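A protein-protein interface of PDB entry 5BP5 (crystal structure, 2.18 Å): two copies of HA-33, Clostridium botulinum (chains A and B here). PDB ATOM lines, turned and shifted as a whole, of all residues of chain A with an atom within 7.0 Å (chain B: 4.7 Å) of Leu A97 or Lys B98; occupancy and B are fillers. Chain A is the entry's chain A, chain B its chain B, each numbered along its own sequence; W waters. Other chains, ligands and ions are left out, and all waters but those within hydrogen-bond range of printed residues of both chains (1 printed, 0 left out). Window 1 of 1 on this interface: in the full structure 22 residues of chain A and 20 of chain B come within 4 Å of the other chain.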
ATOM      1  N   TRP A  94       0.777 -33.036  15.433  1.00  0.00           N
ATOM      2  CA  TRP A  94       0.420 -33.172  14.019  1.00  0.00           C
ATOM      3  C   TRP A  94       0.307 -31.812  13.346  1.00  0.00           C
ATOM      4  O   TRP A  94      -0.162 -30.829  13.959  1.00  0.00           O
ATOM      5  CB  TRP A  94      -0.903 -33.910  13.901  1.00  0.00           C
ATOM      6  CG  TRP A  94      -0.870 -35.157  14.638  1.00  0.00           C
ATOM      7  CD1 TRP A  94      -1.208 -35.341  15.942  1.00  0.00           C
ATOM      8  CD2 TRP A  94      -0.426 -36.423  14.148  1.00  0.00           C
ATOM      9  NE1 TRP A  94      -0.997 -36.637  16.301  1.00  0.00           N
ATOM     10  CE2 TRP A  94      -0.531 -37.333  15.215  1.00  0.00           C
ATOM     11  CE3 TRP A  94       0.012 -36.888  12.891  1.00  0.00           C
ATOM     12  CZ2 TRP A  94      -0.186 -38.661  15.092  1.00  0.00           C
ATOM     13  CZ3 TRP A  94       0.369 -38.202  12.762  1.00  0.00           C
ATOM     14  CH2 TRP A  94       0.249 -39.094  13.848  1.00  0.00           C
ATOM     15  N   LEU A  95       0.780 -31.744  12.105  1.00  0.00           N
ATOM     16  CA  LEU A  95       0.578 -30.568  11.274  1.00  0.00           C
ATOM     17  C   LEU A  95      -0.714 -30.742  10.491  1.00  0.00           C
ATOM     18  O   LEU A  95      -0.908 -31.766   9.841  1.00  0.00           O
ATOM     19  CB  LEU A  95       1.750 -30.364  10.316  1.00  0.00           C
ATOM     20  CG  LEU A  95       3.173 -30.475  10.852  1.00  0.00           C
ATOM     21  CD1 LEU A  95       4.158 -30.123   9.747  1.00  0.00           C
ATOM     22  CD2 LEU A  95       3.410 -29.599  12.068  1.00  0.00           C
ATOM     23  N   LEU A  96      -1.594 -29.748  10.553  1.00  0.00           N
ATOM     24  CA  LEU A  96      -2.832 -29.753   9.782  1.00  0.00           C
ATOM     25  C   LEU A  96      -2.635 -28.896   8.550  1.00  0.00           C
ATOM     26  O   LEU A  96      -2.707 -27.655   8.586  1.00  0.00           O
ATOM     27  CB  LEU A  96      -4.053 -29.293  10.588  1.00  0.00           C
ATOM     28  CG  LEU A  96      -4.226 -30.065  11.888  1.00  0.00           C
ATOM     29  CD1 LEU A  96      -5.479 -29.669  12.642  1.00  0.00           C
ATOM     30  CD2 LEU A  96      -4.228 -31.534  11.653  1.00  0.00           C
ATOM     31  N   LEU A  97      -2.395 -29.582   7.445  1.00  0.00           N
ATOM     32  CA  LEU A  97      -2.124 -28.939   6.183  1.00  0.00           C
ATOM     33  C   LEU A  97      -3.367 -29.006   5.322  1.00  0.00           C
ATOM     34  O   LEU A  97      -3.723 -30.069   4.832  1.00  0.00           O
ATOM     35  CB  LEU A  97      -0.955 -29.641   5.512  1.00  0.00           C
ATOM     36  CG  LEU A  97       0.259 -29.853   6.390  1.00  0.00           C
ATOM     37  CD1 LEU A  97       1.275 -30.705   5.655  1.00  0.00           C
ATOM     38  CD2 LEU A  97       0.851 -28.526   6.758  1.00  0.00           C
ATOM     39  N   LYS A  98      -4.023 -27.868   5.152  1.00  0.00           N
ATOM     40  CA  LYS A  98      -5.242 -27.770   4.358  1.00  0.00           C
ATOM     41  C   LYS A  98      -4.933 -27.689   2.865  1.00  0.00           C
ATOM     42  O   LYS A  98      -4.253 -26.770   2.386  1.00  0.00           O
ATOM     43  CB  LYS A  98      -6.044 -26.541   4.767  1.00  0.00           C
ATOM     44  CG  LYS A  98      -7.518 -26.588   4.409  1.00  0.00           C
ATOM     45  CD  LYS A  98      -8.169 -25.243   4.704  1.00  0.00           C
ATOM     46  CE  LYS A  98      -9.659 -25.338   4.969  1.00  0.00           C
ATOM     47  NZ  LYS A  98     -10.395 -25.777   3.766  1.00  0.00           N
ATOM     48  N   ASP A  99      -5.475 -28.654   2.134  1.00  0.00           N
ATOM     49  CA  ASP A  99      -5.317 -28.710   0.703  1.00  0.00           C
ATOM     50  C   ASP A  99      -6.363 -27.814   0.084  1.00  0.00           C
ATOM     51  O   ASP A  99      -7.491 -28.239  -0.168  1.00  0.00           O
ATOM     52  CB  ASP A  99      -5.474 -30.148   0.256  1.00  0.00           C
ATOM     53  CG  ASP A  99      -5.074 -30.374  -1.190  1.00  0.00           C
ATOM     54  OD1 ASP A  99      -5.202 -29.480  -2.043  1.00  0.00           O
ATOM     55  OD2 ASP A  99      -4.635 -31.498  -1.451  1.00  0.00           O
ATOM     56  N   ILE A 100      -5.973 -26.565  -0.165  1.00  0.00           N
ATOM     57  CA  ILE A 100      -6.888 -25.540  -0.639  1.00  0.00           C
ATOM     58  C   ILE A 100      -7.487 -25.914  -2.007  1.00  0.00           C
ATOM     59  O   ILE A 100      -6.784 -26.359  -2.916  1.00  0.00           O
ATOM     60  CB  ILE A 100      -6.191 -24.162  -0.755  1.00  0.00           C
ATOM     61  CG1 ILE A 100      -5.578 -23.723   0.581  1.00  0.00           C
ATOM     62  CG2 ILE A 100      -7.171 -23.114  -1.239  1.00  0.00           C
ATOM     63  CD1 ILE A 100      -6.509 -23.810   1.769  1.00  0.00           C
ATOM     64  N   SER A 104      -9.782 -30.517   1.932  1.00  0.00           N
ATOM     65  CA  SER A 104      -9.338 -31.665   2.689  1.00  0.00           C
ATOM     66  C   SER A 104      -8.019 -31.310   3.361  1.00  0.00           C
ATOM     67  O   SER A 104      -7.394 -30.320   2.993  1.00  0.00           O
ATOM     68  CB  SER A 104      -9.175 -32.883   1.779  1.00  0.00           C
ATOM     69  OG  SER A 104      -8.367 -32.607   0.632  1.00  0.00           O
ATOM     70  N   PHE A 105      -7.619 -32.129   4.332  1.00  0.00           N
ATOM     71  CA  PHE A 105      -6.377 -31.970   5.042  1.00  0.00           C
ATOM     72  C   PHE A 105      -5.485 -33.162   4.865  1.00  0.00           C
ATOM     73  O   PHE A 105      -5.916 -34.302   4.964  1.00  0.00           O
ATOM     74  CB  PHE A 105      -6.608 -31.819   6.559  1.00  0.00           C
ATOM     75  CG  PHE A 105      -7.179 -30.501   6.972  1.00  0.00           C
ATOM     76  CD1 PHE A 105      -6.383 -29.550   7.626  1.00  0.00           C
ATOM     77  CD2 PHE A 105      -8.530 -30.228   6.789  1.00  0.00           C
ATOM     78  CE1 PHE A 105      -6.926 -28.347   8.017  1.00  0.00           C
ATOM     79  CE2 PHE A 105      -9.077 -29.017   7.191  1.00  0.00           C
ATOM     80  CZ  PHE A 105      -8.272 -28.078   7.813  1.00  0.00           C
ATOM     81  N   ILE A 106      -4.220 -32.881   4.629  1.00  0.00           N
ATOM     82  CA  ILE A 106      -3.167 -33.841   4.898  1.00  0.00           C
ATOM     83  C   ILE A 106      -2.740 -33.642   6.350  1.00  0.00           C
ATOM     84  O   ILE A 106      -2.582 -32.519   6.788  1.00  0.00           O
ATOM     85  CB  ILE A 106      -2.002 -33.680   3.907  1.00  0.00           C
ATOM     86  CG1 ILE A 106      -2.513 -34.080   2.530  1.00  0.00           C
ATOM     87  CG2 ILE A 106      -0.808 -34.516   4.353  1.00  0.00           C
ATOM     88  CD1 ILE A 106      -1.621 -33.775   1.340  1.00  0.00           C
ATOM     89  N   ILE A 107      -2.590 -34.731   7.090  1.00  0.00           N
ATOM     90  CA  ILE A 107      -2.270 -34.686   8.513  1.00  0.00           C
ATOM     91  C   ILE A 107      -0.912 -35.350   8.727  1.00  0.00           C
ATOM     92  O   ILE A 107      -0.797 -36.583   8.786  1.00  0.00           O
ATOM     93  CB  ILE A 107      -3.351 -35.352   9.372  1.00  0.00           C
ATOM     94  CG1 ILE A 107      -4.712 -34.687   9.135  1.00  0.00           C
ATOM     95  CG2 ILE A 107      -3.019 -35.238  10.849  1.00  0.00           C
ATOM     96  CD1 ILE A 107      -5.863 -35.375   9.846  1.00  0.00           C
ATOM     97  N   ALA A 108       0.113 -34.508   8.842  1.00  0.00           N
ATOM     98  CA  ALA A 108       1.495 -34.962   8.937  1.00  0.00           C
ATOM     99  C   ALA A 108       1.992 -35.037  10.386  1.00  0.00           C
ATOM    100  O   ALA A 108       1.608 -34.229  11.196  1.00  0.00           O
ATOM    101  CB  ALA A 108       2.386 -34.048   8.125  1.00  0.00           C
ATOM    102  N   PRO A 113       7.625 -35.210   9.649  1.00  0.00           N
ATOM    103  CA  PRO A 113       6.718 -34.766   8.575  1.00  0.00           C
ATOM    104  C   PRO A 113       6.851 -35.516   7.235  1.00  0.00           C
ATOM    105  O   PRO A 113       6.043 -35.286   6.352  1.00  0.00           O
ATOM    106  CB  PRO A 113       7.075 -33.305   8.397  1.00  0.00           C
ATOM    107  CG  PRO A 113       7.630 -32.892   9.725  1.00  0.00           C
ATOM    108  CD  PRO A 113       8.393 -34.085  10.211  1.00  0.00           C
ATOM    109  N   VAL A 116       2.617 -39.098   6.946  1.00  0.00           N
ATOM    110  CA  VAL A 116       1.263 -38.562   7.058  1.00  0.00           C
ATOM    111  C   VAL A 116       0.271 -39.679   7.365  1.00  0.00           C
ATOM    112  O   VAL A 116       0.547 -40.836   7.112  1.00  0.00           O
ATOM    113  CB  VAL A 116       0.832 -37.795   5.785  1.00  0.00           C
ATOM    114  CG1 VAL A 116       1.881 -36.779   5.403  1.00  0.00           C
ATOM    115  CG2 VAL A 116       0.576 -38.733   4.603  1.00  0.00           C
ATOM    116  N   LEU A 131       4.003 -39.719   1.090  1.00  0.00           N
ATOM    117  CA  LEU A 131       2.927 -38.992   0.417  1.00  0.00           C
ATOM    118  C   LEU A 131       2.618 -39.539  -0.972  1.00  0.00           C
ATOM    119  O   LEU A 131       3.460 -40.147  -1.602  1.00  0.00           O
ATOM    120  CB  LEU A 131       3.274 -37.508   0.305  1.00  0.00           C
ATOM    121  CG  LEU A 131       3.183 -36.781   1.660  1.00  0.00           C
ATOM    122  CD1 LEU A 131       4.520 -36.806   2.345  1.00  0.00           C
ATOM    123  CD2 LEU A 131       2.695 -35.356   1.495  1.00  0.00           C
ATOM    124  N   ILE A 141     -12.031 -32.433   8.053  1.00  0.00           N
ATOM    125  CA  ILE A 141     -12.092 -32.011   9.456  1.00  0.00           C
ATOM    126  C   ILE A 141     -13.191 -30.996   9.555  1.00  0.00           C
ATOM    127  O   ILE A 141     -13.176 -30.003   8.867  1.00  0.00           O
ATOM    128  CB  ILE A 141     -10.779 -31.388   9.947  1.00  0.00           C
ATOM    129  CG1 ILE A 141      -9.666 -32.422   9.880  1.00  0.00           C
ATOM    130  CG2 ILE A 141     -10.944 -30.827  11.366  1.00  0.00           C
ATOM    131  CD1 ILE A 141      -8.289 -31.842  10.024  1.00  0.00           C
ATOM    132  N   LEU B  96      -1.017 -26.811  -3.041  1.00  0.00           N
ATOM    133  CA  LEU B  96      -0.941 -25.687  -2.159  1.00  0.00           C
ATOM    134  C   LEU B  96      -1.545 -26.125  -0.838  1.00  0.00           C
ATOM    135  O   LEU B  96      -2.766 -26.186  -0.682  1.00  0.00           O
ATOM    136  CB  LEU B  96      -1.681 -24.497  -2.743  1.00  0.00           C
ATOM    137  CG  LEU B  96      -1.120 -23.978  -4.069  1.00  0.00           C
ATOM    138  CD1 LEU B  96      -1.861 -22.737  -4.544  1.00  0.00           C
ATOM    139  CD2 LEU B  96       0.372 -23.703  -4.023  1.00  0.00           C
ATOM    140  N   LEU B  97      -0.670 -26.444   0.107  1.00  0.00           N
ATOM    141  CA  LEU B  97      -1.070 -26.939   1.394  1.00  0.00           C
ATOM    142  C   LEU B  97      -0.858 -25.813   2.428  1.00  0.00           C
ATOM    143  O   LEU B  97       0.274 -25.432   2.724  1.00  0.00           O
ATOM    144  CB  LEU B  97      -0.248 -28.184   1.725  1.00  0.00           C
ATOM    145  CG  LEU B  97      -0.164 -29.232   0.615  1.00  0.00           C
ATOM    146  CD1 LEU B  97       0.726 -30.408   0.976  1.00  0.00           C
ATOM    147  CD2 LEU B  97      -1.552 -29.740   0.255  1.00  0.00           C
ATOM    148  N   LYS B  98      -1.959 -25.280   2.952  1.00  0.00           N
ATOM    149  CA  LYS B  98      -1.921 -24.238   3.954  1.00  0.00           C
ATOM    150  C   LYS B  98      -1.752 -24.792   5.370  1.00  0.00           C
ATOM    151  O   LYS B  98      -2.605 -25.512   5.873  1.00  0.00           O
ATOM    152  CB  LYS B  98      -3.186 -23.412   3.901  1.00  0.00           C
ATOM    153  CG  LYS B  98      -3.040 -22.077   4.611  1.00  0.00           C
ATOM    154  CD  LYS B  98      -4.322 -21.298   4.544  1.00  0.00           C
ATOM    155  CE  LYS B  98      -4.105 -19.902   5.056  1.00  0.00           C
ATOM    156  NZ  LYS B  98      -5.411 -19.322   5.431  1.00  0.00           N
ATOM    157  N   ASP B  99      -0.638 -24.457   5.999  1.00  0.00           N
ATOM    158  CA  ASP B  99      -0.387 -24.856   7.392  1.00  0.00           C
ATOM    159  C   ASP B  99      -1.192 -23.964   8.334  1.00  0.00           C
ATOM    160  O   ASP B  99      -0.779 -22.834   8.623  1.00  0.00           O
ATOM    161  CB  ASP B  99       1.110 -24.781   7.669  1.00  0.00           C
ATOM    162  CG  ASP B  99       1.502 -25.335   9.026  1.00  0.00           C
ATOM    163  OD1 ASP B  99       0.651 -25.525   9.902  1.00  0.00           O
ATOM    164  OD2 ASP B  99       2.701 -25.591   9.191  1.00  0.00           O
ATOM    165  N   ILE B 100      -2.327 -24.472   8.809  1.00  0.00           N
ATOM    166  CA  ILE B 100      -3.256 -23.688   9.628  1.00  0.00           C
ATOM    167  C   ILE B 100      -2.643 -23.317  10.985  1.00  0.00           C
ATOM    168  O   ILE B 100      -1.881 -24.084  11.576  1.00  0.00           O
ATOM    169  CB  ILE B 100      -4.608 -24.401   9.868  1.00  0.00           C
ATOM    170  CG1 ILE B 100      -5.291 -24.760   8.550  1.00  0.00           C
ATOM    171  CG2 ILE B 100      -5.548 -23.519  10.669  1.00  0.00           C
ATOM    172  CD1 ILE B 100      -5.489 -23.623   7.587  1.00  0.00           C
ATOM    173  N   ASN B 103      -0.354 -19.777   9.252  1.00  0.00           N
ATOM    174  CA  ASN B 103      -0.688 -18.915   8.124  1.00  0.00           C
ATOM    175  C   ASN B 103       0.370 -18.886   7.002  1.00  0.00           C
ATOM    176  O   ASN B 103       0.686 -17.831   6.456  1.00  0.00           O
ATOM    177  CB  ASN B 103      -0.992 -17.504   8.617  1.00  0.00           C
ATOM    178  CG  ASN B 103      -1.879 -16.738   7.658  1.00  0.00           C
ATOM    179  OD1 ASN B 103      -2.811 -17.307   7.075  1.00  0.00           O
ATOM    180  ND2 ASN B 103      -1.594 -15.448   7.478  1.00  0.00           N
ATOM    181  N   SER B 104       0.907 -20.053   6.670  1.00  0.00           N
ATOM    182  CA  SER B 104       1.862 -20.195   5.586  1.00  0.00           C
ATOM    183  C   SER B 104       1.514 -21.421   4.748  1.00  0.00           C
ATOM    184  O   SER B 104       0.694 -22.241   5.152  1.00  0.00           O
ATOM    185  CB  SER B 104       3.269 -20.350   6.141  1.00  0.00           C
ATOM    186  OG  SER B 104       3.375 -21.550   6.894  1.00  0.00           O
ATOM    187  N   PHE B 105       2.170 -21.543   3.599  1.00  0.00           N
ATOM    188  CA  PHE B 105       1.906 -22.622   2.659  1.00  0.00           C
ATOM    189  C   PHE B 105       3.128 -23.481   2.484  1.00  0.00           C
ATOM    190  O   PHE B 105       4.256 -22.994   2.485  1.00  0.00           O
ATOM    191  CB  PHE B 105       1.485 -22.091   1.291  1.00  0.00           C
ATOM    192  CG  PHE B 105       0.075 -21.577   1.225  1.00  0.00           C
ATOM    193  CD1 PHE B 105      -0.943 -22.386   0.771  1.00  0.00           C
ATOM    194  CD2 PHE B 105      -0.228 -20.258   1.583  1.00  0.00           C
ATOM    195  CE1 PHE B 105      -2.251 -21.925   0.701  1.00  0.00           C
ATOM    196  CE2 PHE B 105      -1.526 -19.780   1.515  1.00  0.00           C
ATOM    197  CZ  PHE B 105      -2.547 -20.621   1.057  1.00  0.00           C
ATOM    198  N   ILE B 106       2.874 -24.774   2.345  1.00  0.00           N
ATOM    199  CA  ILE B 106       3.832 -25.714   1.804  1.00  0.00           C
ATOM    200  C   ILE B 106       3.369 -25.983   0.360  1.00  0.00           C
ATOM    201  O   ILE B 106       2.164 -26.100   0.081  1.00  0.00           O
ATOM    202  CB  ILE B 106       3.925 -26.988   2.677  1.00  0.00           C
ATOM    203  CG1 ILE B 106       4.621 -26.648   3.997  1.00  0.00           C
ATOM    204  CG2 ILE B 106       4.731 -28.053   1.985  1.00  0.00           C
ATOM    205  CD1 ILE B 106       4.350 -27.596   5.146  1.00  0.00           C
HETATM  206  O   HOH W   1      -0.047 -27.380  11.742  1.00  0.00           O
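The backbone carbonyl oxygen of Leu A97 is in hydrogen-bond range of the backbone NH of Ile A106, 2.9 Å away.
The backbone carbonyl oxygen (O) of Ser A104 is in hydrogen-bond range of the backbone NH (N) of Asp A99 (2.7 Å).
The backbone carbonyl oxygen of Leu B97 lies within hydrogen-bond range of the backbone NH of Ile B106.
O of Ser B104 lies within hydrogen-bond range of N of Asp B99, 2.7 Å away.
Trp A94 touches none of the printed residues of chain B.
Leu A97 touches three residues of chain B.
Of the printed residues of chain B, Ile A100 touches Leu B96, Lys B98 and Phe B105.
Of the printed residues of chain A, Leu B96 touches Lys A98 (3.5 Å), Asp A99 (3.8 Å) and Ile A100 (3.3 Å).
Of the printed residues of chain A, Leu B97 touches Lys A98 and Asp A99.
Of the printed residues of chain A, Asp B99 touches Leu A96 and Leu A97.
Ser B104 touches none of the printed residues of chain A.
The nearest residue of chain B that does not touch Leu A97 is Leu B97 (4.1 Å).
The nearest residue of chain A that does not touch Lys B98 is Asp A99 (4.9 Å).
Leu A97 touches Lys B98, and with the chains exchanged Lys A98 touches Leu B97.
Leu A97 touches Ile B106, but with the chains exchanged Ile A106 does not touch Leu B97 (4.1 Å).
Ile A100 touches Lys B98, but with the chains exchanged Lys A98 does not touch Ile B100 (4.1 Å).
Ile A100 touches Phe B105, and with the chains exchanged Phe A105 touches Ile B100.
Positions printed for both chains: 96, 97, 98, 99, 100, 104, 105 and 106.
Of the 15 pairs that touch across the chains among the printed residues, 13 have their exchanged pair printed and touching as well.
Along chain A the printed residues that touch a printed residue of chain B span positions 96 to 105.
Water W1 bridges OD1 of Asp B99 and N of Leu A96.
O of Leu A96 sits at hydrogen-bond distance from N of Ile B100, at 3.2 Å.
O of Lys A98 lies within hydrogen-bond range of N of Lys B98.
O of Leu B96 sits at hydrogen-bond distance from N of Ile A100 (3.3 Å).
The backbone carbonyl oxygen of Leu A96 sits close to the backbone carbonyl oxygen of Lys B98 (3.5 Å).
O of Leu B96 sits close to O of Lys A98 (3.5 Å).
O of Leu A96 touches CA of Asp B99 (3.8 Å).
Leu A97 touches Lys B98.
CD2 of Leu A97 touches CB of Asp B99, at 3.9 Å.
Leu A97 touches Ile B106 (CD2 to CD1, 3.96 Å).
Lys A98 touches Leu B97 (O to CA, 3.3 Å).
Leu B96 touches Asp A99 (O to CA, 3.8 Å).
Leu B97 touches Asp A99.
Lys B98 touches Ile A100 (CB to CD1, 3.97 Å).
Ile A100 touches Phe B105 (CG1 to CE1, 3.8 Å).
Ile B100 touches Phe A105.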
